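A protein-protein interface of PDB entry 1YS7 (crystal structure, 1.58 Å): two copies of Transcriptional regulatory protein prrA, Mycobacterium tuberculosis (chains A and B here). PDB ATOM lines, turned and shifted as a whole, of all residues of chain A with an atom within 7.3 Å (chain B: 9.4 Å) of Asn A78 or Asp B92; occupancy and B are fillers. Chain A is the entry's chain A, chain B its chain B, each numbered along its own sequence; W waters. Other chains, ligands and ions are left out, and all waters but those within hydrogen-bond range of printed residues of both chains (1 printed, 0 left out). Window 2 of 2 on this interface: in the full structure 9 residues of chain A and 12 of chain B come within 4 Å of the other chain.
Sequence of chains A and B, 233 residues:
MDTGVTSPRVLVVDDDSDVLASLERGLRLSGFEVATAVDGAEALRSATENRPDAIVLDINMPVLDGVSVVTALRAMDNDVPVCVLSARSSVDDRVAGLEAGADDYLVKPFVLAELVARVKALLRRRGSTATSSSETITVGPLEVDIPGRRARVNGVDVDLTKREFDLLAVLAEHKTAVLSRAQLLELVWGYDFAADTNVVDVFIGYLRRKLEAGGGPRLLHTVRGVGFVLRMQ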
ATOM      1  N   LEU A  44      -0.202   4.051  33.878  1.00  0.00           N
ATOM      2  CA  LEU A  44       0.038   3.028  32.854  1.00  0.00           C
ATOM      3  C   LEU A  44       0.907   1.898  33.353  1.00  0.00           C
ATOM      4  O   LEU A  44       0.646   0.733  33.030  1.00  0.00           O
ATOM      5  CB  LEU A  44       0.637   3.626  31.593  1.00  0.00           C
ATOM      6  CG  LEU A  44      -0.309   4.469  30.752  1.00  0.00           C
ATOM      7  CD1 LEU A  44       0.487   5.088  29.602  1.00  0.00           C
ATOM      8  CD2 LEU A  44      -1.522   3.607  30.223  1.00  0.00           C
ATOM      9  N   ALA A  47      -1.386  -0.158  35.732  1.00  0.00           N
ATOM     10  CA  ALA A  47      -2.441  -0.851  34.978  1.00  0.00           C
ATOM     11  C   ALA A  47      -1.869  -2.088  34.284  1.00  0.00           C
ATOM     12  O   ALA A  47      -2.596  -3.094  34.075  1.00  0.00           O
ATOM     13  CB  ALA A  47      -3.128   0.099  33.978  1.00  0.00           C
ATOM     14  N   THR A  48      -0.575  -1.997  33.955  1.00  0.00           N
ATOM     15  CA  THR A  48       0.218  -3.084  33.337  1.00  0.00           C
ATOM     16  C   THR A  48       0.662  -4.140  34.338  1.00  0.00           C
ATOM     17  O   THR A  48       0.475  -5.356  34.113  1.00  0.00           O
ATOM     18  CB  THR A  48       1.441  -2.478  32.615  1.00  0.00           C
ATOM     19  OG1 THR A  48       0.955  -1.798  31.465  1.00  0.00           O
ATOM     20  CG2 THR A  48       2.484  -3.553  32.193  1.00  0.00           C
ATOM     21  N   ARG A  51      -3.151  -5.508  36.615  1.00  0.00           N
ATOM     22  CA  ARG A  51      -4.430  -5.346  35.908  1.00  0.00           C
ATOM     23  C   ARG A  51      -5.637  -5.010  36.813  1.00  0.00           C
ATOM     24  O   ARG A  51      -6.300  -5.905  37.334  1.00  0.00           O
ATOM     25  CB  ARG A  51      -4.716  -6.629  35.113  1.00  0.00           C
ATOM     26  CG  ARG A  51      -3.561  -7.115  34.198  1.00  0.00           C
ATOM     27  CD  ARG A  51      -3.336  -8.646  34.250  1.00  0.00           C
ATOM     28  NE  ARG A  51      -3.046  -9.158  32.907  1.00  0.00           N
ATOM     29  CZ  ARG A  51      -3.803 -10.023  32.228  1.00  0.00           C
ATOM     30  NH1 ARG A  51      -4.905 -10.552  32.764  1.00  0.00           N
ATOM     31  NH2 ARG A  51      -3.429 -10.389  31.004  1.00  0.00           N
ATOM     32  N   PRO A  52      -5.969  -3.714  36.982  1.00  0.00           N
ATOM     33  CA  PRO A  52      -7.085  -3.376  37.861  1.00  0.00           C
ATOM     34  C   PRO A  52      -8.413  -3.681  37.221  1.00  0.00           C
ATOM     35  O   PRO A  52      -8.484  -3.767  35.991  1.00  0.00           O
ATOM     36  CB  PRO A  52      -6.963  -1.856  38.019  1.00  0.00           C
ATOM     37  CG  PRO A  52      -6.213  -1.400  36.825  1.00  0.00           C
ATOM     38  CD  PRO A  52      -5.340  -2.517  36.379  1.00  0.00           C
ATOM     39  N   ILE A  55     -10.529   1.785  36.851  1.00  0.00           N
ATOM     40  CA  ILE A  55      -9.571   2.932  37.034  1.00  0.00           C
ATOM     41  C   ILE A  55     -10.328   4.225  37.279  1.00  0.00           C
ATOM     42  O   ILE A  55     -11.256   4.529  36.565  1.00  0.00           O
ATOM     43  CB  ILE A  55      -8.617   3.119  35.820  1.00  0.00           C
ATOM     44  CG1 ILE A  55      -7.779   1.850  35.556  1.00  0.00           C
ATOM     45  CG2 ILE A  55      -7.644   4.291  36.044  1.00  0.00           C
ATOM     46  CD1 ILE A  55      -6.872   1.946  34.384  1.00  0.00           C
ATOM     47  N   VAL A  70      -6.208   7.665  28.889  1.00  0.00           N
ATOM     48  CA  VAL A  70      -7.392   7.017  28.255  1.00  0.00           C
ATOM     49  C   VAL A  70      -7.069   6.720  26.813  1.00  0.00           C
ATOM     50  O   VAL A  70      -7.252   5.587  26.365  1.00  0.00           O
ATOM     51  CB  VAL A  70      -8.654   7.945  28.345  1.00  0.00           C
ATOM     52  CG1 VAL A  70      -9.830   7.367  27.539  1.00  0.00           C
ATOM     53  CG2 VAL A  70      -8.973   8.104  29.784  1.00  0.00           C
ATOM     54  N   ALA A  72      -4.245   6.259  25.376  1.00  0.00           N
ATOM     55  CA  ALA A  72      -3.226   5.214  25.240  1.00  0.00           C
ATOM     56  C   ALA A  72      -3.861   3.869  25.575  1.00  0.00           C
ATOM     57  O   ALA A  72      -3.631   2.918  24.833  1.00  0.00           O
ATOM     58  CB  ALA A  72      -2.040   5.521  26.188  1.00  0.00           C
ATOM     59  N   LEU A  73      -4.660   3.792  26.646  1.00  0.00           N
ATOM     60  CA  LEU A  73      -5.291   2.504  27.032  1.00  0.00           C
ATOM     61  C   LEU A  73      -6.132   1.981  25.870  1.00  0.00           C
ATOM     62  O   LEU A  73      -6.061   0.786  25.493  1.00  0.00           O
ATOM     63  CB  LEU A  73      -6.160   2.660  28.267  1.00  0.00           C
ATOM     64  CG  LEU A  73      -5.423   2.873  29.579  1.00  0.00           C
ATOM     65  CD1 LEU A  73      -6.456   3.230  30.614  1.00  0.00           C
ATOM     66  CD2 LEU A  73      -4.694   1.618  29.977  1.00  0.00           C
ATOM     67  N   ARG A  74      -6.962   2.864  25.317  1.00  0.00           N
ATOM     68  CA  ARG A  74      -7.859   2.402  24.258  1.00  0.00           C
ATOM     69  C   ARG A  74      -7.101   2.044  23.005  1.00  0.00           C
ATOM     70  O   ARG A  74      -7.456   1.066  22.283  1.00  0.00           O
ATOM     71  CB  ARG A  74      -8.936   3.442  23.986  1.00  0.00           C
ATOM     72  CG  ARG A  74      -9.759   3.795  25.222  1.00  0.00           C
ATOM     73  CD  ARG A  74     -10.251   2.541  25.971  1.00  0.00           C
ATOM     74  NE  ARG A  74     -11.257   2.888  26.951  1.00  0.00           N
ATOM     75  CZ  ARG A  74     -11.354   2.377  28.172  1.00  0.00           C
ATOM     76  NH1 ARG A  74     -10.480   1.472  28.616  1.00  0.00           N
ATOM     77  NH2 ARG A  74     -12.362   2.787  28.966  1.00  0.00           N
ATOM     78  N   ALA A  75      -6.022   2.793  22.732  1.00  0.00           N
ATOM     79  CA  ALA A  75      -5.212   2.550  21.525  1.00  0.00           C
ATOM     80  C   ALA A  75      -4.572   1.155  21.606  1.00  0.00           C
ATOM     81  O   ALA A  75      -4.374   0.474  20.586  1.00  0.00           O
ATOM     82  CB  ALA A  75      -4.115   3.597  21.398  1.00  0.00           C
ATOM     83  N   MET A  76      -4.271   0.761  22.817  1.00  0.00           N
ATOM     84  CA  MET A  76      -3.650  -0.523  23.110  1.00  0.00           C
ATOM     85  C   MET A  76      -4.677  -1.617  23.325  1.00  0.00           C
ATOM     86  O   MET A  76      -4.312  -2.707  23.803  1.00  0.00           O
ATOM     87  CB  MET A  76      -2.720  -0.402  24.306  1.00  0.00           C
ATOM     88  CG  MET A  76      -1.522   0.492  24.020  1.00  0.00           C
ATOM     89  SD  MET A  76      -0.331   0.678  25.369  1.00  0.00           S
ATOM     90  CE  MET A  76      -1.255   1.679  26.607  1.00  0.00           C
ATOM     91  N   ASP A  77      -5.933  -1.333  22.962  1.00  0.00           N
ATOM     92  CA  ASP A  77      -7.019  -2.333  23.028  1.00  0.00           C
ATOM     93  C   ASP A  77      -7.291  -2.767  24.462  1.00  0.00           C
ATOM     94  O   ASP A  77      -7.676  -3.926  24.722  1.00  0.00           O
ATOM     95  CB  ASP A  77      -6.729  -3.559  22.112  1.00  0.00           C
ATOM     96  CG  ASP A  77      -6.381  -3.168  20.711  1.00  0.00           C
ATOM     97  OD1 ASP A  77      -7.137  -2.342  20.137  1.00  0.00           O
ATOM     98  OD2 ASP A  77      -5.362  -3.716  20.169  1.00  0.00           O
ATOM     99  N   ASN A  78      -7.071  -1.859  25.410  1.00  0.00           N
ATOM    100  CA  ASN A  78      -7.375  -2.120  26.802  1.00  0.00           C
ATOM    101  C   ASN A  78      -8.721  -1.569  27.202  1.00  0.00           C
ATOM    102  O   ASN A  78      -8.852  -0.346  27.356  1.00  0.00           O
ATOM    103  CB  ASN A  78      -6.287  -1.572  27.709  1.00  0.00           C
ATOM    104  CG  ASN A  78      -6.433  -2.062  29.172  1.00  0.00           C
ATOM    105  OD1 ASN A  78      -7.531  -2.387  29.621  1.00  0.00           O
ATOM    106  ND2 ASN A  78      -5.313  -2.108  29.898  1.00  0.00           N
ATOM    107  N   ASP A  79      -9.686  -2.460  27.429  1.00  0.00           N
ATOM    108  CA  ASP A  79     -11.043  -2.027  27.679  1.00  0.00           C
ATOM    109  C   ASP A  79     -11.377  -1.877  29.161  1.00  0.00           C
ATOM    110  O   ASP A  79     -12.559  -1.790  29.524  1.00  0.00           O
ATOM    111  CB  ASP A  79     -12.058  -2.915  26.965  1.00  0.00           C
ATOM    112  CG  ASP A  79     -12.110  -2.642  25.459  1.00  0.00           C
ATOM    113  OD1 ASP A  79     -11.844  -1.505  24.996  1.00  0.00           O
ATOM    114  OD2 ASP A  79     -12.409  -3.598  24.728  1.00  0.00           O
ATOM    115  N   VAL A  80     -10.331  -1.733  29.966  1.00  0.00           N
ATOM    116  CA  VAL A  80     -10.500  -1.575  31.409  1.00  0.00           C
ATOM    117  C   VAL A  80     -11.523  -0.465  31.653  1.00  0.00           C
ATOM    118  O   VAL A  80     -11.463   0.592  30.990  1.00  0.00           O
ATOM    119  CB  VAL A  80      -9.172  -1.270  32.116  1.00  0.00           C
ATOM    120  CG1 VAL A  80      -8.558   0.028  31.563  1.00  0.00           C
ATOM    121  CG2 VAL A  80      -9.377  -1.255  33.647  1.00  0.00           C
ATOM    122  N   PRO A  81     -12.489  -0.659  32.576  1.00  0.00           N
ATOM    123  CA  PRO A  81     -13.414   0.414  32.918  1.00  0.00           C
ATOM    124  C   PRO A  81     -12.709   1.659  33.457  1.00  0.00           C
ATOM    125  O   PRO A  81     -11.837   1.506  34.310  1.00  0.00           O
ATOM    126  CB  PRO A  81     -14.322  -0.222  33.985  1.00  0.00           C
ATOM    127  CG  PRO A  81     -14.240  -1.713  33.630  1.00  0.00           C
ATOM    128  CD  PRO A  81     -12.843  -1.904  33.295  1.00  0.00           C
ATOM    129  N   VAL A  82     -13.077   2.869  32.982  1.00  0.00           N
ATOM    130  CA  VAL A  82     -12.447   4.073  33.463  1.00  0.00           C
ATOM    131  C   VAL A  82     -13.467   5.145  33.808  1.00  0.00           C
ATOM    132  O   VAL A  82     -14.308   5.497  32.988  1.00  0.00           O
ATOM    133  CB  VAL A  82     -11.441   4.662  32.414  1.00  0.00           C
ATOM    134  CG1 VAL A  82     -10.895   6.082  32.847  1.00  0.00           C
ATOM    135  CG2 VAL A  82     -10.311   3.708  32.209  1.00  0.00           C
ATOM    136  N   GLY A 101     -12.467   8.073  25.359  1.00  0.00           N
ATOM    137  CA  GLY A 101     -12.716   6.652  25.640  1.00  0.00           C
ATOM    138  C   GLY A 101     -13.072   6.273  27.070  1.00  0.00           C
ATOM    139  O   GLY A 101     -13.297   5.109  27.338  1.00  0.00           O
ATOM    140  N   LYS A 162     -15.757   2.318  23.371  1.00  0.00           N
ATOM    141  CA  LYS A 162     -16.407   1.134  23.927  1.00  0.00           C
ATOM    142  C   LYS A 162     -17.803   1.509  24.470  1.00  0.00           C
ATOM    143  O   LYS A 162     -18.828   0.891  24.124  1.00  0.00           O
ATOM    144  CB  LYS A 162     -15.519   0.561  25.057  1.00  0.00           C
ATOM    145  CG  LYS A 162     -16.033  -0.690  25.757  1.00  0.00           C
ATOM    146  CD  LYS A 162     -15.179  -0.928  27.011  1.00  0.00           C
ATOM    147  CE  LYS A 162     -15.514   0.166  28.035  1.00  0.00           C
ATOM    148  NZ  LYS A 162     -14.934   0.018  29.428  1.00  0.00           N
ATOM    149  N   ILE B  59     -14.219 -16.227  19.352  1.00  0.00           N
ATOM    150  CA  ILE B  59     -14.601 -15.731  20.680  1.00  0.00           C
ATOM    151  C   ILE B  59     -15.918 -14.930  20.664  1.00  0.00           C
ATOM    152  O   ILE B  59     -16.814 -15.153  21.491  1.00  0.00           O
ATOM    153  CB  ILE B  59     -13.524 -14.856  21.265  1.00  0.00           C
ATOM    154  CG1 ILE B  59     -12.289 -15.698  21.526  1.00  0.00           C
ATOM    155  CG2 ILE B  59     -14.028 -14.200  22.583  1.00  0.00           C
ATOM    156  CD1 ILE B  59     -12.448 -16.607  22.721  1.00  0.00           C
ATOM    157  N   ASN B  60     -16.012 -13.989  19.726  1.00  0.00           N
ATOM    158  CA  ASN B  60     -17.151 -13.098  19.690  1.00  0.00           C
ATOM    159  C   ASN B  60     -18.232 -13.619  18.779  1.00  0.00           C
ATOM    160  O   ASN B  60     -18.126 -13.533  17.529  1.00  0.00           O
ATOM    161  CB  ASN B  60     -16.644 -11.763  19.245  1.00  0.00           C
ATOM    162  CG  ASN B  60     -15.706 -11.174  20.272  1.00  0.00           C
ATOM    163  OD1 ASN B  60     -16.061 -11.093  21.451  1.00  0.00           O
ATOM    164  ND2 ASN B  60     -14.499 -10.838  19.864  1.00  0.00           N
ATOM    165  N   VAL B  67     -15.848 -17.442  25.122  1.00  0.00           N
ATOM    166  CA  VAL B  67     -15.430 -17.528  26.551  1.00  0.00           C
ATOM    167  C   VAL B  67     -16.394 -18.426  27.299  1.00  0.00           C
ATOM    168  O   VAL B  67     -15.976 -19.308  28.064  1.00  0.00           O
ATOM    169  CB  VAL B  67     -15.298 -16.145  27.176  1.00  0.00           C
ATOM    170  CG1 VAL B  67     -14.876 -16.264  28.673  1.00  0.00           C
ATOM    171  CG2 VAL B  67     -14.265 -15.381  26.386  1.00  0.00           C
ATOM    172  N   VAL B  84      -8.669 -20.657  20.176  1.00  0.00           N
ATOM    173  CA  VAL B  84      -9.658 -19.572  19.999  1.00  0.00           C
ATOM    174  C   VAL B  84      -9.203 -18.574  18.937  1.00  0.00           C
ATOM    175  O   VAL B  84      -7.989 -18.323  18.759  1.00  0.00           O
ATOM    176  CB  VAL B  84      -9.953 -18.842  21.324  1.00  0.00           C
ATOM    177  CG1 VAL B  84     -10.682 -19.755  22.358  1.00  0.00           C
ATOM    178  CG2 VAL B  84      -8.703 -18.205  21.894  1.00  0.00           C
ATOM    179  N   SER B  86      -9.762 -14.658  17.213  1.00  0.00           N
ATOM    180  CA  SER B  86     -10.320 -13.325  17.441  1.00  0.00           C
ATOM    181  C   SER B  86      -9.694 -12.311  16.519  1.00  0.00           C
ATOM    182  O   SER B  86      -8.630 -12.558  16.002  1.00  0.00           O
ATOM    183  CB  SER B  86     -10.092 -12.890  18.886  1.00  0.00           C
ATOM    184  OG  SER B  86      -8.720 -12.760  19.196  1.00  0.00           O
ATOM    185  N   ALA B  87     -10.353 -11.156  16.349  1.00  0.00           N
ATOM    186  CA  ALA B  87      -9.801 -10.040  15.575  1.00  0.00           C
ATOM    187  C   ALA B  87      -8.611  -9.486  16.296  1.00  0.00           C
ATOM    188  O   ALA B  87      -8.561  -9.579  17.508  1.00  0.00           O
ATOM    189  CB  ALA B  87     -10.861  -8.947  15.418  1.00  0.00           C
ATOM    190  N   ARG B  88      -7.668  -8.902  15.547  1.00  0.00           N
ATOM    191  CA  ARG B  88      -6.386  -8.432  16.119  1.00  0.00           C
ATOM    192  C   ARG B  88      -6.589  -7.501  17.307  1.00  0.00           C
ATOM    193  O   ARG B  88      -5.809  -7.501  18.264  1.00  0.00           O
ATOM    194  CB  ARG B  88      -5.531  -7.733  15.059  1.00  0.00           C
ATOM    195  CG  ARG B  88      -4.048  -7.873  15.308  1.00  0.00           C
ATOM    196  CD  ARG B  88      -3.333  -7.983  13.949  1.00  0.00           C
ATOM    197  NE  ARG B  88      -1.950  -8.414  14.095  1.00  0.00           N
ATOM    198  CZ  ARG B  88      -1.454  -9.554  13.626  1.00  0.00           C
ATOM    199  NH1 ARG B  88      -2.226 -10.403  12.952  1.00  0.00           N
ATOM    200  NH2 ARG B  88      -0.169  -9.831  13.821  1.00  0.00           N
ATOM    201  N   SER B  89      -7.643  -6.705  17.239  1.00  0.00           N
ATOM    202  CA  SER B  89      -7.864  -5.665  18.262  1.00  0.00           C
ATOM    203  C   SER B  89      -8.576  -6.182  19.494  1.00  0.00           C
ATOM    204  O   SER B  89      -8.606  -5.503  20.533  1.00  0.00           O
ATOM    205  CB  SER B  89      -8.650  -4.471  17.690  1.00  0.00           C
ATOM    206  OG  SER B  89      -7.824  -3.698  16.825  1.00  0.00           O
ATOM    207  N   SER B  90      -9.147  -7.380  19.405  1.00  0.00           N
ATOM    208  CA  SER B  90      -9.928  -7.893  20.502  1.00  0.00           C
ATOM    209  C   SER B  90      -9.029  -8.642  21.508  1.00  0.00           C
ATOM    210  O   SER B  90      -9.226  -9.837  21.789  1.00  0.00           O
ATOM    211  CB  SER B  90     -11.030  -8.790  19.959  1.00  0.00           C
ATOM    212  OG  SER B  90     -11.732  -8.114  18.906  1.00  0.00           O
ATOM    213  N   VAL B  91      -8.044  -7.936  22.040  1.00  0.00           N
ATOM    214  CA  VAL B  91      -7.070  -8.519  22.973  1.00  0.00           C
ATOM    215  C   VAL B  91      -7.749  -9.116  24.208  1.00  0.00           C
ATOM    216  O   VAL B  91      -7.525 -10.320  24.560  1.00  0.00           O
ATOM    217  CB  VAL B  91      -6.029  -7.456  23.443  1.00  0.00           C
ATOM    218  CG1 VAL B  91      -5.034  -8.080  24.425  1.00  0.00           C
ATOM    219  CG2 VAL B  91      -5.301  -6.887  22.277  1.00  0.00           C
ATOM    220  N   ASP B  92      -8.560  -8.295  24.872  1.00  0.00           N
ATOM    221  CA  ASP B  92      -9.152  -8.672  26.151  1.00  0.00           C
ATOM    222  C   ASP B  92      -9.962  -9.973  26.023  1.00  0.00           C
ATOM    223  O   ASP B  92      -9.946 -10.789  26.917  1.00  0.00           O
ATOM    224  CB  ASP B  92      -9.984  -7.521  26.772  1.00  0.00           C
ATOM    225  CG  ASP B  92      -9.098  -6.329  27.277  1.00  0.00           C
ATOM    226  OD1 ASP B  92      -7.862  -6.487  27.402  1.00  0.00           O
ATOM    227  OD2 ASP B  92      -9.661  -5.246  27.561  1.00  0.00           O
ATOM    228  N   ASP B  93     -10.603 -10.146  24.869  1.00  0.00           N
ATOM    229  CA  ASP B  93     -11.479 -11.276  24.585  1.00  0.00           C
ATOM    230  C   ASP B  93     -10.690 -12.559  24.443  1.00  0.00           C
ATOM    231  O   ASP B  93     -11.067 -13.573  25.060  1.00  0.00           O
ATOM    232  CB  ASP B  93     -12.186 -11.029  23.248  1.00  0.00           C
ATOM    233  CG  ASP B  93     -13.167  -9.873  23.307  1.00  0.00           C
ATOM    234  OD1 ASP B  93     -13.089  -8.988  22.418  1.00  0.00           O
ATOM    235  OD2 ASP B  93     -13.995  -9.847  24.248  1.00  0.00           O
ATOM    236  N   ARG B  94      -9.649 -12.559  23.598  1.00  0.00           N
ATOM    237  CA  ARG B  94      -8.870 -13.792  23.450  1.00  0.00           C
ATOM    238  C   ARG B  94      -8.123 -14.135  24.736  1.00  0.00           C
ATOM    239  O   ARG B  94      -8.029 -15.312  25.129  1.00  0.00           O
ATOM    240  CB  ARG B  94      -7.947 -13.788  22.209  1.00  0.00           C
ATOM    241  CG  ARG B  94      -6.914 -12.697  22.154  1.00  0.00           C
ATOM    242  CD  ARG B  94      -5.968 -12.925  20.967  1.00  0.00           C
ATOM    243  NE  ARG B  94      -5.178 -11.736  20.644  1.00  0.00           N
ATOM    244  CZ  ARG B  94      -5.590 -10.682  19.929  1.00  0.00           C
ATOM    245  NH1 ARG B  94      -6.805 -10.619  19.422  1.00  0.00           N
ATOM    246  NH2 ARG B  94      -4.749  -9.691  19.692  1.00  0.00           N
ATOM    247  N   VAL B  95      -7.642 -13.122  25.443  1.00  0.00           N
ATOM    248  CA  VAL B  95      -7.005 -13.394  26.758  1.00  0.00           C
ATOM    249  C   VAL B  95      -8.026 -14.032  27.726  1.00  0.00           C
ATOM    250  O   VAL B  95      -7.718 -15.022  28.451  1.00  0.00           O
ATOM    251  CB  VAL B  95      -6.371 -12.133  27.359  1.00  0.00           C
ATOM    252  CG1 VAL B  95      -6.079 -12.330  28.887  1.00  0.00           C
ATOM    253  CG2 VAL B  95      -5.111 -11.695  26.559  1.00  0.00           C
ATOM    254  N   ALA B  96      -9.262 -13.523  27.700  1.00  0.00           N
ATOM    255  CA  ALA B  96     -10.299 -14.088  28.512  1.00  0.00           C
ATOM    256  C   ALA B  96     -10.494 -15.549  28.096  1.00  0.00           C
ATOM    257  O   ALA B  96     -10.705 -16.406  28.959  1.00  0.00           O
ATOM    258  CB  ALA B  96     -11.610 -13.308  28.308  1.00  0.00           C
ATOM    259  N   GLY B  97     -10.450 -15.850  26.798  1.00  0.00           N
ATOM    260  CA  GLY B  97     -10.668 -17.240  26.405  1.00  0.00           C
ATOM    261  C   GLY B  97      -9.536 -18.161  26.838  1.00  0.00           C
ATOM    262  O   GLY B  97      -9.801 -19.268  27.294  1.00  0.00           O
ATOM    263  N   LEU B  98      -8.286 -17.670  26.778  1.00  0.00           N
ATOM    264  CA  LEU B  98      -7.139 -18.416  27.298  1.00  0.00           C
ATOM    265  C   LEU B  98      -7.266 -18.603  28.794  1.00  0.00           C
ATOM    266  O   LEU B  98      -7.072 -19.712  29.329  1.00  0.00           O
ATOM    267  CB  LEU B  98      -5.821 -17.699  26.961  1.00  0.00           C
ATOM    268  CG  LEU B  98      -5.599 -17.549  25.445  1.00  0.00           C
ATOM    269  CD1 LEU B  98      -4.376 -16.654  25.252  1.00  0.00           C
ATOM    270  CD2 LEU B  98      -5.385 -18.946  24.867  1.00  0.00           C
ATOM    271  N   GLU B  99      -7.582 -17.520  29.511  1.00  0.00           N
ATOM    272  CA  GLU B  99      -7.733 -17.646  30.972  1.00  0.00           C
ATOM    273  C   GLU B  99      -8.817 -18.648  31.392  1.00  0.00           C
ATOM    274  O   GLU B  99      -8.718 -19.283  32.457  1.00  0.00           O
ATOM    275  CB  GLU B  99      -7.950 -16.286  31.677  1.00  0.00           C
ATOM    276  CG  GLU B  99      -6.758 -15.369  31.581  1.00  0.00           C
ATOM    277  CD  GLU B  99      -6.960 -13.968  32.234  1.00  0.00           C
ATOM    278  OE1 GLU B  99      -8.077 -13.677  32.767  1.00  0.00           O
ATOM    279  OE2 GLU B  99      -5.976 -13.176  32.166  1.00  0.00           O
ATOM    280  N   ALA B 100      -9.856 -18.794  30.569  1.00  0.00           N
ATOM    281  CA  ALA B 100     -11.009 -19.644  30.890  1.00  0.00           C
ATOM    282  C   ALA B 100     -10.675 -21.071  30.578  1.00  0.00           C
ATOM    283  O   ALA B 100     -11.372 -21.967  31.018  1.00  0.00           O
ATOM    284  CB  ALA B 100     -12.178 -19.224  30.096  1.00  0.00           C
ATOM    285  N   TYR B 206       0.005 -15.654  33.446  1.00  0.00           N
ATOM    286  CA  TYR B 206      -1.115 -16.219  34.219  1.00  0.00           C
ATOM    287  C   TYR B 206      -0.545 -17.148  35.283  1.00  0.00           C
ATOM    288  O   TYR B 206      -0.943 -17.126  36.437  1.00  0.00           O
ATOM    289  CB  TYR B 206      -2.049 -17.094  33.356  1.00  0.00           C
ATOM    290  CG  TYR B 206      -2.627 -16.465  32.117  1.00  0.00           C
ATOM    291  CD1 TYR B 206      -2.809 -15.090  32.027  1.00  0.00           C
ATOM    292  CD2 TYR B 206      -2.979 -17.265  31.036  1.00  0.00           C
ATOM    293  CE1 TYR B 206      -3.339 -14.519  30.887  1.00  0.00           C
ATOM    294  CE2 TYR B 206      -3.493 -16.720  29.900  1.00  0.00           C
ATOM    295  CZ  TYR B 206      -3.687 -15.346  29.825  1.00  0.00           C
ATOM    296  OH  TYR B 206      -4.211 -14.815  28.649  1.00  0.00           O
HETATM  297  O   HOH W   1      -9.358  -5.684  23.900  1.00  0.00           O
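Hydrophobic or aromatic side chains of chain B within 4 Å of the printed part of chain A: Val B91 and Val B95. Of the 20 printed residues of chain A, 4 touch a printed residue of chain B. Among the printed residues, 7 pairs touch across the chains.
Val B95 touches Arg A51. Ser B89 touches Asp A77 (O to CB, 3.1 Å). CB of Asp A77 touches CG2 of Val B91 (3.6 Å). Asp A77 touches Asp B92. Asn A78 touches Asp B92.
Of the printed residues of chain B, Asn A78 touches Asp B92 (3.8 Å). Of chain A, only Asp A77, Asn A78 and Asp A79 come within 4 Å of Asp B92. No residue of chain B comes within 4 Å of Arg A74. Asp A79 touches one residue of chain B. No residue of chain B comes within 4 Å of Val A80. Of the printed residues of chain B, Asp A77 touches Ser B89, Val B91 and Asp B92. Of the printed residues of chain A, Val B95 touches Arg A51 (3.9 Å). Of the printed residues of chain B, Arg A51 touches Val B95 (3.9 Å) and Glu B99 (2.9 Å). Printed residues of chain A within 4 Å of Glu B99: Arg A51 (2.9 Å).
No position is printed for both chains. Of the 7 pairs that touch across the chains among the printed residues, none has its exchanged pair printed and touching as well.
Water W1 lies within hydrogen-bond range of the backbone carbonyl oxygen (O) of Asp A77 (2.6 Å), the backbone NH (N) of Asp B92 (2.9 Å), the backbone NH (N) of Val B91 (3.2 Å) and the backbone carbonyl oxygen (O) of Ser B89 (3.5 Å).
The guanidinium group (NH1) of Arg A51 is in salt-bridge range of the side-chain carboxylate (OE2) of Glu B99, at 2.9 Å. The backbone NH of Asp A79 is in hydrogen-bond range of the side-chain carboxylate of Asp B92.
The backbone carbonyl oxygen of Leu A73 lies within hydrogen-bond range of the backbone NH of Asn A78. O of Asn A78 lies within hydrogen-bond range of NH1 of Arg A74, at 2.7 Å. The backbone NH of Val A80 sits at hydrogen-bond distance from the side-chain amide oxygen of Asn A78, 2.9 Å away. The backbone carbonyl oxygen (O) of Asp A79 lies within hydrogen-bond range of the side-chain amino group (NZ) of Lys A162 (3.0 Å).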
